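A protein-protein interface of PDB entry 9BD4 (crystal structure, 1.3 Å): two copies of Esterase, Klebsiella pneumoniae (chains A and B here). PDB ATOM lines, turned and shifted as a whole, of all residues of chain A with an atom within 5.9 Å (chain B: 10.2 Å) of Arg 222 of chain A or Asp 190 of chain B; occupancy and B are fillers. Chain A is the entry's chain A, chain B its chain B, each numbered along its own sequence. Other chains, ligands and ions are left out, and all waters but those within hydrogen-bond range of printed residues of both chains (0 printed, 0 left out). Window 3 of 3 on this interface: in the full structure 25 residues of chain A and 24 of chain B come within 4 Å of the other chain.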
ATOM      1  N   MET A 141      12.077  -1.464 -13.423  1.00  0.00           N
ATOM      2  CA  MET A 141      13.458  -1.022 -13.648  1.00  0.00           C
ATOM      3  C   MET A 141      14.474  -2.043 -13.146  1.00  0.00           C
ATOM      4  O   MET A 141      15.426  -1.717 -12.419  1.00  0.00           O
ATOM      5  CB  MET A 141      13.818   0.364 -13.081  1.00  0.00           C
ATOM      6  CG  MET A 141      13.490   0.677 -11.631  1.00  0.00           C
ATOM      7  SD  MET A 141      13.539   2.459 -11.333  1.00  0.00           S
ATOM      8  CE  MET A 141      13.523   2.444  -9.536  1.00  0.00           C
ATOM      9  N   TRP A 184       8.287  -3.024 -16.415  1.00  0.00           N
ATOM     10  CA  TRP A 184       8.233  -1.571 -16.537  1.00  0.00           C
ATOM     11  C   TRP A 184       9.653  -1.039 -16.530  1.00  0.00           C
ATOM     12  O   TRP A 184      10.491  -1.536 -15.778  1.00  0.00           O
ATOM     13  CB  TRP A 184       7.445  -0.928 -15.376  1.00  0.00           C
ATOM     14  CG  TRP A 184       7.356   0.577 -15.507  1.00  0.00           C
ATOM     15  CD1 TRP A 184       6.378   1.289 -16.142  1.00  0.00           C
ATOM     16  CD2 TRP A 184       8.300   1.545 -15.008  1.00  0.00           C
ATOM     17  NE1 TRP A 184       6.665   2.631 -16.080  1.00  0.00           N
ATOM     18  CE2 TRP A 184       7.843   2.815 -15.399  1.00  0.00           C
ATOM     19  CE3 TRP A 184       9.503   1.450 -14.291  1.00  0.00           C
ATOM     20  CZ2 TRP A 184       8.527   3.997 -15.067  1.00  0.00           C
ATOM     21  CZ3 TRP A 184      10.177   2.611 -13.963  1.00  0.00           C
ATOM     22  CH2 TRP A 184       9.694   3.865 -14.349  1.00  0.00           C
ATOM     23  N   GLY A 186      11.921   2.925 -17.244  1.00  0.00           N
ATOM     24  CA  GLY A 186      12.091   4.247 -17.833  1.00  0.00           C
ATOM     25  C   GLY A 186      13.108   4.164 -18.961  1.00  0.00           C
ATOM     26  O   GLY A 186      14.148   3.517 -18.829  1.00  0.00           O
ATOM     27  N   ASP A 187      12.802   4.823 -20.082  1.00  0.00           N
ATOM     28  CA  ASP A 187      13.665   4.642 -21.248  1.00  0.00           C
ATOM     29  C   ASP A 187      14.960   5.435 -21.172  1.00  0.00           C
ATOM     30  O   ASP A 187      15.781   5.338 -22.093  1.00  0.00           O
ATOM     31  CB  ASP A 187      12.913   4.825 -22.580  1.00  0.00           C
ATOM     32  CG  ASP A 187      12.672   6.275 -22.963  1.00  0.00           C
ATOM     33  OD1 ASP A 187      13.144   7.207 -22.284  1.00  0.00           O
ATOM     34  OD2 ASP A 187      11.974   6.484 -23.986  1.00  0.00           O
ATOM     35  N   ALA A 188      15.169   6.201 -20.094  1.00  0.00           N
ATOM     36  CA  ALA A 188      16.386   6.977 -19.876  1.00  0.00           C
ATOM     37  C   ALA A 188      17.134   6.513 -18.626  1.00  0.00           C
ATOM     38  O   ALA A 188      17.959   7.262 -18.084  1.00  0.00           O
ATOM     39  CB  ALA A 188      16.078   8.477 -19.808  1.00  0.00           C
ATOM     40  N   ASP A 189      16.875   5.291 -18.169  1.00  0.00           N
ATOM     41  CA  ASP A 189      17.508   4.792 -16.954  1.00  0.00           C
ATOM     42  C   ASP A 189      19.028   4.780 -17.114  1.00  0.00           C
ATOM     43  O   ASP A 189      19.562   4.252 -18.097  1.00  0.00           O
ATOM     44  CB  ASP A 189      16.950   3.396 -16.655  1.00  0.00           C
ATOM     45  CG  ASP A 189      17.248   2.917 -15.241  1.00  0.00           C
ATOM     46  OD1 ASP A 189      18.371   3.156 -14.741  1.00  0.00           O
ATOM     47  OD2 ASP A 189      16.352   2.285 -14.636  1.00  0.00           O
ATOM     48  N   ASP A 190      19.728   5.429 -16.179  1.00  0.00           N
ATOM     49  CA  ASP A 190      21.186   5.521 -16.204  1.00  0.00           C
ATOM     50  C   ASP A 190      21.844   4.644 -15.139  1.00  0.00           C
ATOM     51  O   ASP A 190      23.043   4.808 -14.869  1.00  0.00           O
ATOM     52  CB  ASP A 190      21.655   6.987 -16.091  1.00  0.00           C
ATOM     53  CG  ASP A 190      21.086   7.709 -14.868  1.00  0.00           C
ATOM     54  OD1 ASP A 190      20.478   7.054 -13.996  1.00  0.00           O
ATOM     55  OD2 ASP A 190      21.236   8.960 -14.809  1.00  0.00           O
ATOM     56  N   GLY A 220      11.642   9.337 -21.284  1.00  0.00           N
ATOM     57  CA  GLY A 220      12.381  10.356 -20.567  1.00  0.00           C
ATOM     58  C   GLY A 220      12.642  10.085 -19.104  1.00  0.00           C
ATOM     59  O   GLY A 220      13.302  10.908 -18.458  1.00  0.00           O
ATOM     60  N   VAL A 221      12.165   8.979 -18.559  1.00  0.00           N
ATOM     61  CA  VAL A 221      12.279   8.706 -17.133  1.00  0.00           C
ATOM     62  C   VAL A 221      13.574   7.947 -16.876  1.00  0.00           C
ATOM     63  O   VAL A 221      13.912   7.011 -17.613  1.00  0.00           O
ATOM     64  CB  VAL A 221      11.042   7.920 -16.648  1.00  0.00           C
ATOM     65  CG1 VAL A 221      11.200   7.460 -15.206  1.00  0.00           C
ATOM     66  CG2 VAL A 221       9.792   8.784 -16.794  1.00  0.00           C
ATOM     67  N   ARG A 222      14.300   8.343 -15.822  1.00  0.00           N
ATOM     68  CA  ARG A 222      15.548   7.676 -15.449  1.00  0.00           C
ATOM     69  C   ARG A 222      15.266   6.584 -14.417  1.00  0.00           C
ATOM     70  O   ARG A 222      14.237   5.909 -14.518  1.00  0.00           O
ATOM     71  CB  ARG A 222      16.617   8.696 -15.035  1.00  0.00           C
ATOM     72  CG  ARG A 222      16.875   9.748 -16.116  1.00  0.00           C
ATOM     73  CD  ARG A 222      18.124  10.565 -15.821  1.00  0.00           C
ATOM     74  NE  ARG A 222      17.900  11.491 -14.718  1.00  0.00           N
ATOM     75  CZ  ARG A 222      18.857  12.183 -14.112  1.00  0.00           C
ATOM     76  NH1 ARG A 222      20.110  12.142 -14.534  1.00  0.00           N
ATOM     77  NH2 ARG A 222      18.545  12.959 -13.073  1.00  0.00           N
ATOM     78  N   HIS A 223      16.158   6.378 -13.442  1.00  0.00           N
ATOM     79  CA  HIS A 223      15.997   5.285 -12.475  1.00  0.00           C
ATOM     80  C   HIS A 223      15.145   5.739 -11.292  1.00  0.00           C
ATOM     81  O   HIS A 223      15.627   5.946 -10.173  1.00  0.00           O
ATOM     82  CB  HIS A 223      17.354   4.764 -12.018  1.00  0.00           C
ATOM     83  CG  HIS A 223      17.286   3.432 -11.340  1.00  0.00           C
ATOM     84  ND1 HIS A 223      17.007   2.265 -12.019  1.00  0.00           N
ATOM     85  CD2 HIS A 223      17.473   3.081 -10.044  1.00  0.00           C
ATOM     86  CE1 HIS A 223      17.020   1.250 -11.170  1.00  0.00           C
ATOM     87  NE2 HIS A 223      17.303   1.720  -9.967  1.00  0.00           N
ATOM     88  N   ARG A 224      13.855   5.900 -11.563  1.00  0.00           N
ATOM     89  CA  ARG A 224      12.928   6.346 -10.533  1.00  0.00           C
ATOM     90  C   ARG A 224      11.511   5.885 -10.849  1.00  0.00           C
ATOM     91  O   ARG A 224      11.097   5.865 -12.014  1.00  0.00           O
ATOM     92  CB  ARG A 224      12.944   7.868 -10.379  1.00  0.00           C
ATOM     93  CG  ARG A 224      12.501   8.611 -11.592  1.00  0.00           C
ATOM     94  CD  ARG A 224      11.890   9.958 -11.192  1.00  0.00           C
ATOM     95  NE  ARG A 224      11.498  10.736 -12.361  1.00  0.00           N
ATOM     96  CZ  ARG A 224      10.343  11.371 -12.495  1.00  0.00           C
ATOM     97  NH1 ARG A 224       9.440  11.383 -11.522  1.00  0.00           N
ATOM     98  NH2 ARG A 224      10.089  12.021 -13.627  1.00  0.00           N
ATOM     99  N   ILE A 225      10.764   5.556  -9.797  1.00  0.00           N
ATOM    100  CA  ILE A 225       9.362   5.171  -9.926  1.00  0.00           C
ATOM    101  C   ILE A 225       8.499   6.431  -9.952  1.00  0.00           C
ATOM    102  O   ILE A 225       8.545   7.258  -9.036  1.00  0.00           O
ATOM    103  CB  ILE A 225       8.944   4.250  -8.773  1.00  0.00           C
ATOM    104  CG1 ILE A 225       9.830   2.996  -8.724  1.00  0.00           C
ATOM    105  CG2 ILE A 225       7.472   3.882  -8.900  1.00  0.00           C
ATOM    106  CD1 ILE A 225       9.789   2.149  -9.991  1.00  0.00           C
ATOM    107  N   THR B  40       6.435  16.575 -10.653  1.00  0.00           N
ATOM    108  CA  THR B  40       5.981  15.425 -11.453  1.00  0.00           C
ATOM    109  C   THR B  40       5.757  14.172 -10.617  1.00  0.00           C
ATOM    110  O   THR B  40       5.435  13.109 -11.187  1.00  0.00           O
ATOM    111  CB  THR B  40       6.813  15.111 -12.713  1.00  0.00           C
ATOM    112  OG1 THR B  40       8.038  14.466 -12.342  1.00  0.00           O
ATOM    113  CG2 THR B  40       7.103  16.371 -13.520  1.00  0.00           C
ATOM    114  N   SER B 118      12.591  18.228  -2.653  1.00  0.00           N
ATOM    115  CA  SER B 118      12.743  18.802  -4.000  1.00  0.00           C
ATOM    116  C   SER B 118      11.847  20.034  -4.109  1.00  0.00           C
ATOM    117  O   SER B 118      11.977  20.959  -3.289  1.00  0.00           O
ATOM    118  CB  SER B 118      12.513  17.717  -5.036  1.00  0.00           C
ATOM    119  OG  SER B 118      13.058  18.098  -6.289  1.00  0.00           O
ATOM    120  N   MET B 141      16.868  17.928  -0.422  1.00  0.00           N
ATOM    121  CA  MET B 141      17.272  18.089  -1.823  1.00  0.00           C
ATOM    122  C   MET B 141      16.497  19.185  -2.548  1.00  0.00           C
ATOM    123  O   MET B 141      15.980  19.006  -3.657  1.00  0.00           O
ATOM    124  CB  MET B 141      17.321  16.766  -2.600  1.00  0.00           C
ATOM    125  CG  MET B 141      16.103  15.872  -2.523  1.00  0.00           C
ATOM    126  SD  MET B 141      16.380  14.311  -3.388  1.00  0.00           S
ATOM    127  CE  MET B 141      14.683  13.869  -3.810  1.00  0.00           C
ATOM    128  N   LEU B 149      17.377  30.250  -9.171  1.00  0.00           N
ATOM    129  CA  LEU B 149      17.210  28.883  -9.651  1.00  0.00           C
ATOM    130  C   LEU B 149      16.194  28.801 -10.789  1.00  0.00           C
ATOM    131  O   LEU B 149      16.288  27.909 -11.644  1.00  0.00           O
ATOM    132  CB  LEU B 149      16.841  27.954  -8.487  1.00  0.00           C
ATOM    133  CG  LEU B 149      16.821  26.443  -8.759  1.00  0.00           C
ATOM    134  CD1 LEU B 149      18.148  25.953  -9.332  1.00  0.00           C
ATOM    135  CD2 LEU B 149      16.477  25.694  -7.482  1.00  0.00           C
ATOM    136  N   THR B 152      17.461  28.347 -14.433  1.00  0.00           N
ATOM    137  CA  THR B 152      18.145  27.138 -14.881  1.00  0.00           C
ATOM    138  C   THR B 152      17.356  25.848 -14.692  1.00  0.00           C
ATOM    139  O   THR B 152      17.455  24.958 -15.538  1.00  0.00           O
ATOM    140  CB  THR B 152      19.533  27.011 -14.221  1.00  0.00           C
ATOM    141  OG1 THR B 152      19.389  26.829 -12.809  1.00  0.00           O
ATOM    142  CG2 THR B 152      20.383  28.249 -14.494  1.00  0.00           C
ATOM    143  N   LEU B 153      16.561  25.726 -13.637  1.00  0.00           N
ATOM    144  CA  LEU B 153      15.806  24.510 -13.363  1.00  0.00           C
ATOM    145  C   LEU B 153      14.364  24.711 -13.816  1.00  0.00           C
ATOM    146  O   LEU B 153      13.672  25.585 -13.293  1.00  0.00           O
ATOM    147  CB  LEU B 153      15.855  24.195 -11.872  1.00  0.00           C
ATOM    148  CG  LEU B 153      15.000  23.023 -11.398  1.00  0.00           C
ATOM    149  CD1 LEU B 153      15.542  21.704 -11.916  1.00  0.00           C
ATOM    150  CD2 LEU B 153      14.911  23.015  -9.878  1.00  0.00           C
ATOM    151  N   PHE B 154      13.917  23.894 -14.775  1.00  0.00           N
ATOM    152  CA  PHE B 154      12.590  23.980 -15.380  1.00  0.00           C
ATOM    153  C   PHE B 154      12.113  25.431 -15.554  1.00  0.00           C
ATOM    154  O   PHE B 154      11.078  25.810 -15.000  1.00  0.00           O
ATOM    155  CB  PHE B 154      11.561  23.164 -14.602  1.00  0.00           C
ATOM    156  CG  PHE B 154      11.864  21.690 -14.517  1.00  0.00           C
ATOM    157  CD1 PHE B 154      11.769  20.885 -15.644  1.00  0.00           C
ATOM    158  CD2 PHE B 154      12.210  21.108 -13.308  1.00  0.00           C
ATOM    159  CE1 PHE B 154      12.026  19.520 -15.563  1.00  0.00           C
ATOM    160  CE2 PHE B 154      12.471  19.749 -13.225  1.00  0.00           C
ATOM    161  CZ  PHE B 154      12.384  18.960 -14.351  1.00  0.00           C
ATOM    162  N   HIS B 185      20.978  17.114   1.727  1.00  0.00           N
ATOM    163  CA  HIS B 185      21.235  17.050   0.287  1.00  0.00           C
ATOM    164  C   HIS B 185      22.235  15.937   0.006  1.00  0.00           C
ATOM    165  O   HIS B 185      23.192  15.754   0.761  1.00  0.00           O
ATOM    166  CB  HIS B 185      21.832  18.377  -0.209  1.00  0.00           C
ATOM    167  CG  HIS B 185      21.301  18.832  -1.531  1.00  0.00           C
ATOM    168  ND1 HIS B 185      20.615  20.020  -1.673  1.00  0.00           N
ATOM    169  CD2 HIS B 185      21.292  18.242  -2.752  1.00  0.00           C
ATOM    170  CE1 HIS B 185      20.235  20.159  -2.933  1.00  0.00           C
ATOM    171  NE2 HIS B 185      20.625  19.090  -3.607  1.00  0.00           N
ATOM    172  N   GLY B 186      22.006  15.196  -1.078  1.00  0.00           N
ATOM    173  CA  GLY B 186      23.031  14.292  -1.601  1.00  0.00           C
ATOM    174  C   GLY B 186      24.050  15.074  -2.423  1.00  0.00           C
ATOM    175  O   GLY B 186      23.676  15.931  -3.230  1.00  0.00           O
ATOM    176  N   ASP B 187      25.333  14.805  -2.200  1.00  0.00           N
ATOM    177  CA  ASP B 187      26.335  15.672  -2.821  1.00  0.00           C
ATOM    178  C   ASP B 187      26.610  15.360  -4.286  1.00  0.00           C
ATOM    179  O   ASP B 187      27.487  15.995  -4.884  1.00  0.00           O
ATOM    180  CB  ASP B 187      27.607  15.812  -1.969  1.00  0.00           C
ATOM    181  CG  ASP B 187      28.517  14.598  -2.026  1.00  0.00           C
ATOM    182  OD1 ASP B 187      28.284  13.675  -2.833  1.00  0.00           O
ATOM    183  OD2 ASP B 187      29.489  14.569  -1.234  1.00  0.00           O
ATOM    184  N   ALA B 188      25.883  14.410  -4.885  1.00  0.00           N
ATOM    185  CA  ALA B 188      26.009  14.112  -6.306  1.00  0.00           C
ATOM    186  C   ALA B 188      24.707  14.411  -7.036  1.00  0.00           C
ATOM    187  O   ALA B 188      24.498  13.921  -8.149  1.00  0.00           O
ATOM    188  CB  ALA B 188      26.435  12.659  -6.528  1.00  0.00           C
ATOM    189  N   ASP B 189      23.825  15.197  -6.419  1.00  0.00           N
ATOM    190  CA  ASP B 189      22.525  15.496  -7.008  1.00  0.00           C
ATOM    191  C   ASP B 189      22.704  16.251  -8.326  1.00  0.00           C
ATOM    192  O   ASP B 189      23.305  17.328  -8.356  1.00  0.00           O
ATOM    193  CB  ASP B 189      21.715  16.314  -5.998  1.00  0.00           C
ATOM    194  CG  ASP B 189      20.246  16.451  -6.368  1.00  0.00           C
ATOM    195  OD1 ASP B 189      19.905  16.526  -7.563  1.00  0.00           O
ATOM    196  OD2 ASP B 189      19.429  16.511  -5.415  1.00  0.00           O
ATOM    197  N   ASP B 190      22.162  15.690  -9.409  1.00  0.00           N
ATOM    198  CA  ASP B 190      22.271  16.260 -10.748  1.00  0.00           C
ATOM    199  C   ASP B 190      20.968  16.893 -11.216  1.00  0.00           C
ATOM    200  O   ASP B 190      20.828  17.201 -12.409  1.00  0.00           O
ATOM    201  CB  ASP B 190      22.768  15.210 -11.751  1.00  0.00           C
ATOM    202  CG  ASP B 190      21.850  13.999 -11.870  1.00  0.00           C
ATOM    203  OD1 ASP B 190      20.887  13.861 -11.091  1.00  0.00           O
ATOM    204  OD2 ASP B 190      22.106  13.169 -12.767  1.00  0.00           O
ATOM    205  N   VAL B 191      20.009  17.069 -10.311  1.00  0.00           N
ATOM    206  CA  VAL B 191      18.738  17.734 -10.606  1.00  0.00           C
ATOM    207  C   VAL B 191      18.660  19.088  -9.908  1.00  0.00           C
ATOM    208  O   VAL B 191      18.560  20.135 -10.560  1.00  0.00           O
ATOM    209  CB  VAL B 191      17.540  16.832 -10.234  1.00  0.00           C
ATOM    210  CG1 VAL B 191      16.202  17.544 -10.520  1.00  0.00           C
ATOM    211  CG2 VAL B 191      17.633  15.487 -10.970  1.00  0.00           C
ATOM    212  N   VAL B 192      18.718  19.089  -8.580  1.00  0.00           N
ATOM    213  CA  VAL B 192      18.905  20.302  -7.790  1.00  0.00           C
ATOM    214  C   VAL B 192      20.347  20.285  -7.292  1.00  0.00           C
ATOM    215  O   VAL B 192      20.680  19.459  -6.428  1.00  0.00           O
ATOM    216  CB  VAL B 192      17.928  20.368  -6.606  1.00  0.00           C
ATOM    217  CG1 VAL B 192      18.142  21.671  -5.833  1.00  0.00           C
ATOM    218  CG2 VAL B 192      16.481  20.249  -7.074  1.00  0.00           C
ATOM    219  N   PRO B 193      21.224  21.153  -7.793  1.00  0.00           N
ATOM    220  CA  PRO B 193      22.653  21.084  -7.425  1.00  0.00           C
ATOM    221  C   PRO B 193      22.849  21.198  -5.923  1.00  0.00           C
ATOM    222  O   PRO B 193      22.195  22.024  -5.262  1.00  0.00           O
ATOM    223  CB  PRO B 193      23.239  22.310  -8.139  1.00  0.00           C
ATOM    224  CG  PRO B 193      22.332  22.495  -9.333  1.00  0.00           C
ATOM    225  CD  PRO B 193      20.962  22.206  -8.791  1.00  0.00           C
ATOM    226  N   PRO B 194      23.750  20.394  -5.345  1.00  0.00           N
ATOM    227  CA  PRO B 194      24.028  20.529  -3.901  1.00  0.00           C
ATOM    228  C   PRO B 194      24.548  21.900  -3.518  1.00  0.00           C
ATOM    229  O   PRO B 194      24.397  22.309  -2.354  1.00  0.00           O
ATOM    230  CB  PRO B 194      25.066  19.431  -3.621  1.00  0.00           C
ATOM    231  CG  PRO B 194      25.637  19.074  -4.956  1.00  0.00           C
ATOM    232  CD  PRO B 194      24.573  19.348  -5.980  1.00  0.00           C
ATOM    233  N   GLU B 195      25.118  22.641  -4.472  1.00  0.00           N
ATOM    234  CA  GLU B 195      25.541  24.009  -4.205  1.00  0.00           C
ATOM    235  C   GLU B 195      24.401  24.874  -3.680  1.00  0.00           C
ATOM    236  O   GLU B 195      24.656  25.840  -2.958  1.00  0.00           O
ATOM    237  CB  GLU B 195      26.125  24.625  -5.473  1.00  0.00           C
ATOM    238  CG  GLU B 195      27.516  24.105  -5.846  1.00  0.00           C
ATOM    239  CD  GLU B 195      27.521  22.814  -6.679  1.00  0.00           C
ATOM    240  OE1 GLU B 195      26.462  22.184  -6.894  1.00  0.00           O
ATOM    241  OE2 GLU B 195      28.622  22.428  -7.133  1.00  0.00           O
ATOM    242  N   GLU B 196      23.146  24.554  -4.019  1.00  0.00           N
ATOM    243  CA  GLU B 196      22.023  25.324  -3.480  1.00  0.00           C
ATOM    244  C   GLU B 196      22.006  25.279  -1.957  1.00  0.00           C
ATOM    245  O   GLU B 196      21.823  26.305  -1.292  1.00  0.00           O
ATOM    246  CB  GLU B 196      20.691  24.801  -4.033  1.00  0.00           C
ATOM    247  CG  GLU B 196      20.544  24.894  -5.545  1.00  0.00           C
ATOM    248  CD  GLU B 196      20.642  26.313  -6.083  1.00  0.00           C
ATOM    249  OE1 GLU B 196      19.788  27.148  -5.719  1.00  0.00           O
ATOM    250  OE2 GLU B 196      21.561  26.601  -6.884  1.00  0.00           O
ATOM    251  N   GLY B 220      28.017  10.954  -2.322  1.00  0.00           N
ATOM    252  CA  GLY B 220      27.752  10.091  -3.462  1.00  0.00           C
ATOM    253  C   GLY B 220      26.293   9.947  -3.850  1.00  0.00           C
ATOM    254  O   GLY B 220      26.002   9.323  -4.879  1.00  0.00           O
ATOM    255  N   VAL B 221      25.369  10.508  -3.084  1.00  0.00           N
ATOM    256  CA  VAL B 221      23.940  10.306  -3.295  1.00  0.00           C
ATOM    257  C   VAL B 221      23.426  11.320  -4.310  1.00  0.00           C
ATOM    258  O   VAL B 221      23.781  12.505  -4.269  1.00  0.00           O
ATOM    259  CB  VAL B 221      23.182  10.397  -1.953  1.00  0.00           C
ATOM    260  CG1 VAL B 221      21.676  10.401  -2.165  1.00  0.00           C
ATOM    261  CG2 VAL B 221      23.585   9.213  -1.057  1.00  0.00           C
ATOM    262  N   ARG B 222      22.593  10.848  -5.240  1.00  0.00           N
ATOM    263  CA  ARG B 222      22.033  11.718  -6.272  1.00  0.00           C
ATOM    264  C   ARG B 222      20.688  12.299  -5.812  1.00  0.00           C
ATOM    265  O   ARG B 222      20.507  12.551  -4.614  1.00  0.00           O
ATOM    266  CB  ARG B 222      21.973  10.946  -7.596  1.00  0.00           C
ATOM    267  CG  ARG B 222      23.358  10.464  -8.038  1.00  0.00           C
ATOM    268  CD  ARG B 222      23.315   9.526  -9.246  1.00  0.00           C
ATOM    269  NE  ARG B 222      22.761  10.191 -10.420  1.00  0.00           N
ATOM    270  CZ  ARG B 222      22.206   9.561 -11.446  1.00  0.00           C
ATOM    271  NH1 ARG B 222      22.184   8.239 -11.517  1.00  0.00           N
ATOM    272  NH2 ARG B 222      21.661  10.277 -12.424  1.00  0.00           N
ATOM    273  N   HIS B 223      19.752  12.535  -6.733  1.00  0.00           N
ATOM    274  CA  HIS B 223      18.465  13.149  -6.392  1.00  0.00           C
ATOM    275  C   HIS B 223      17.510  12.050  -5.932  1.00  0.00           C
ATOM    276  O   HIS B 223      16.553  11.673  -6.612  1.00  0.00           O
ATOM    277  CB  HIS B 223      17.915  13.919  -7.585  1.00  0.00           C
ATOM    278  CG  HIS B 223      16.819  14.879  -7.230  1.00  0.00           C
ATOM    279  ND1 HIS B 223      17.031  15.991  -6.445  1.00  0.00           N
ATOM    280  CD2 HIS B 223      15.504  14.888  -7.555  1.00  0.00           C
ATOM    281  CE1 HIS B 223      15.889  16.645  -6.296  1.00  0.00           C
ATOM    282  NE2 HIS B 223      14.951  16.001  -6.972  1.00  0.00           N
ATOM    283  N   ARG B 224      17.805  11.525  -4.745  1.00  0.00           N
ATOM    284  CA  ARG B 224      17.105  10.361  -4.229  1.00  0.00           C
ATOM    285  C   ARG B 224      17.093  10.406  -2.707  1.00  0.00           C
ATOM    286  O   ARG B 224      18.112  10.710  -2.078  1.00  0.00           O
ATOM    287  CB  ARG B 224      17.820   9.088  -4.698  1.00  0.00           C
ATOM    288  CG  ARG B 224      17.425   7.829  -3.972  1.00  0.00           C
ATOM    289  CD  ARG B 224      16.144   7.285  -4.560  1.00  0.00           C
ATOM    290  NE  ARG B 224      15.836   5.960  -4.046  1.00  0.00           N
ATOM    291  CZ  ARG B 224      16.087   4.833  -4.695  1.00  0.00           C
ATOM    292  NH1 ARG B 224      16.621   4.838  -5.905  1.00  0.00           N
ATOM    293  NH2 ARG B 224      15.799   3.673  -4.115  1.00  0.00           N
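The side-chain hydroxyl (OG1) of Thr 40 of chain B sits at hydrogen-bond distance from the guanidinium group (NH2) of Arg 224 of chain A (3.4 Å).
NH2 of Arg 222 of chain B lies close to NH1 of Arg 222 of chain A (3.2 Å).
NH1 of Arg 222 of chain A is in salt-bridge range of OD2 of Asp 190 of chain B.
The side-chain carboxylate of Asp 190 of chain A is in salt-bridge range of the guanidinium group of Arg 222 of chain B (2.8 Å).
SD of Met 141 of chain A sits at hydrogen-bond distance from N of Arg 224 of chain A (3.5 Å).
The side-chain carboxylate (OD2) of Asp 190 of chain B lies within salt-bridge range of the guanidinium group (NH2) of Arg 222 of chain B (2.9 Å).
OD2 of Asp 190 of chain A lies within salt-bridge range of NH1 of Arg 222 of chain A.
OD1 of Asp 189 of chain B sits at hydrogen-bond distance from N of Val 191 of chain B, at 2.8 Å.
Among the printed residues, merely in contact across the chains: Arg 222 of chain A with Val 191 of chain B.
No residue of chain B comes within 4 Å of Gly 186 of chain A.
No residue of chain B comes within 4 Å of Ala 188 of chain A.
Of the printed residues of chain B, Asp 190 of chain A touches Arg 222.
Of chain B, only Asp 190, Val 191 and Arg 222 come within 4 Å of Arg 222 of chain A.
Of the printed residues of chain B, Arg 224 of chain A touches Thr 40.
Of the printed residues of chain A, Thr 40 of chain B touches Arg 224.
Of chain A, only Arg 222 (2.9 Å) comes within 4 Å of Asp 190 of chain B.
Printed residues of chain A within 4 Å of Arg 222 of chain B: Asp 190 (2.8 Å) and Arg 222 (3.2 Å).
The nearest residue of chain B that does not touch Arg 222 of chain A is His 223 of chain B (5.6 Å).
The nearest residue of chain A that does not touch Asp 190 of chain B is Asp 190 of chain A (4.8 Å).
The nearest printed residue of chain B that does not touch Arg 224 of chain A is Arg 224 of chain B (6.1 Å).
Of the 24 printed residues of chain B, 4 touch a printed residue of chain A.
Among the printed residues, 5 pairs touch across the chains.
Among the printed residues, Asp or Glu carboxylates within 4 Å of a Lys or Arg side-chain nitrogen of the other chain: Asp 190 of chain A with Arg 222 of chain B (2.8 Å) and Arg 222 of chain A with Asp 190 of chain B (2.9 Å).
Asp 190 of chain A touches Arg 222 of chain B, and with the chains exchanged Arg 222 of chain A touches Asp 190 of chain B.
Arg 222 of chain B touches its own counterpart, Arg 222 of chain A.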
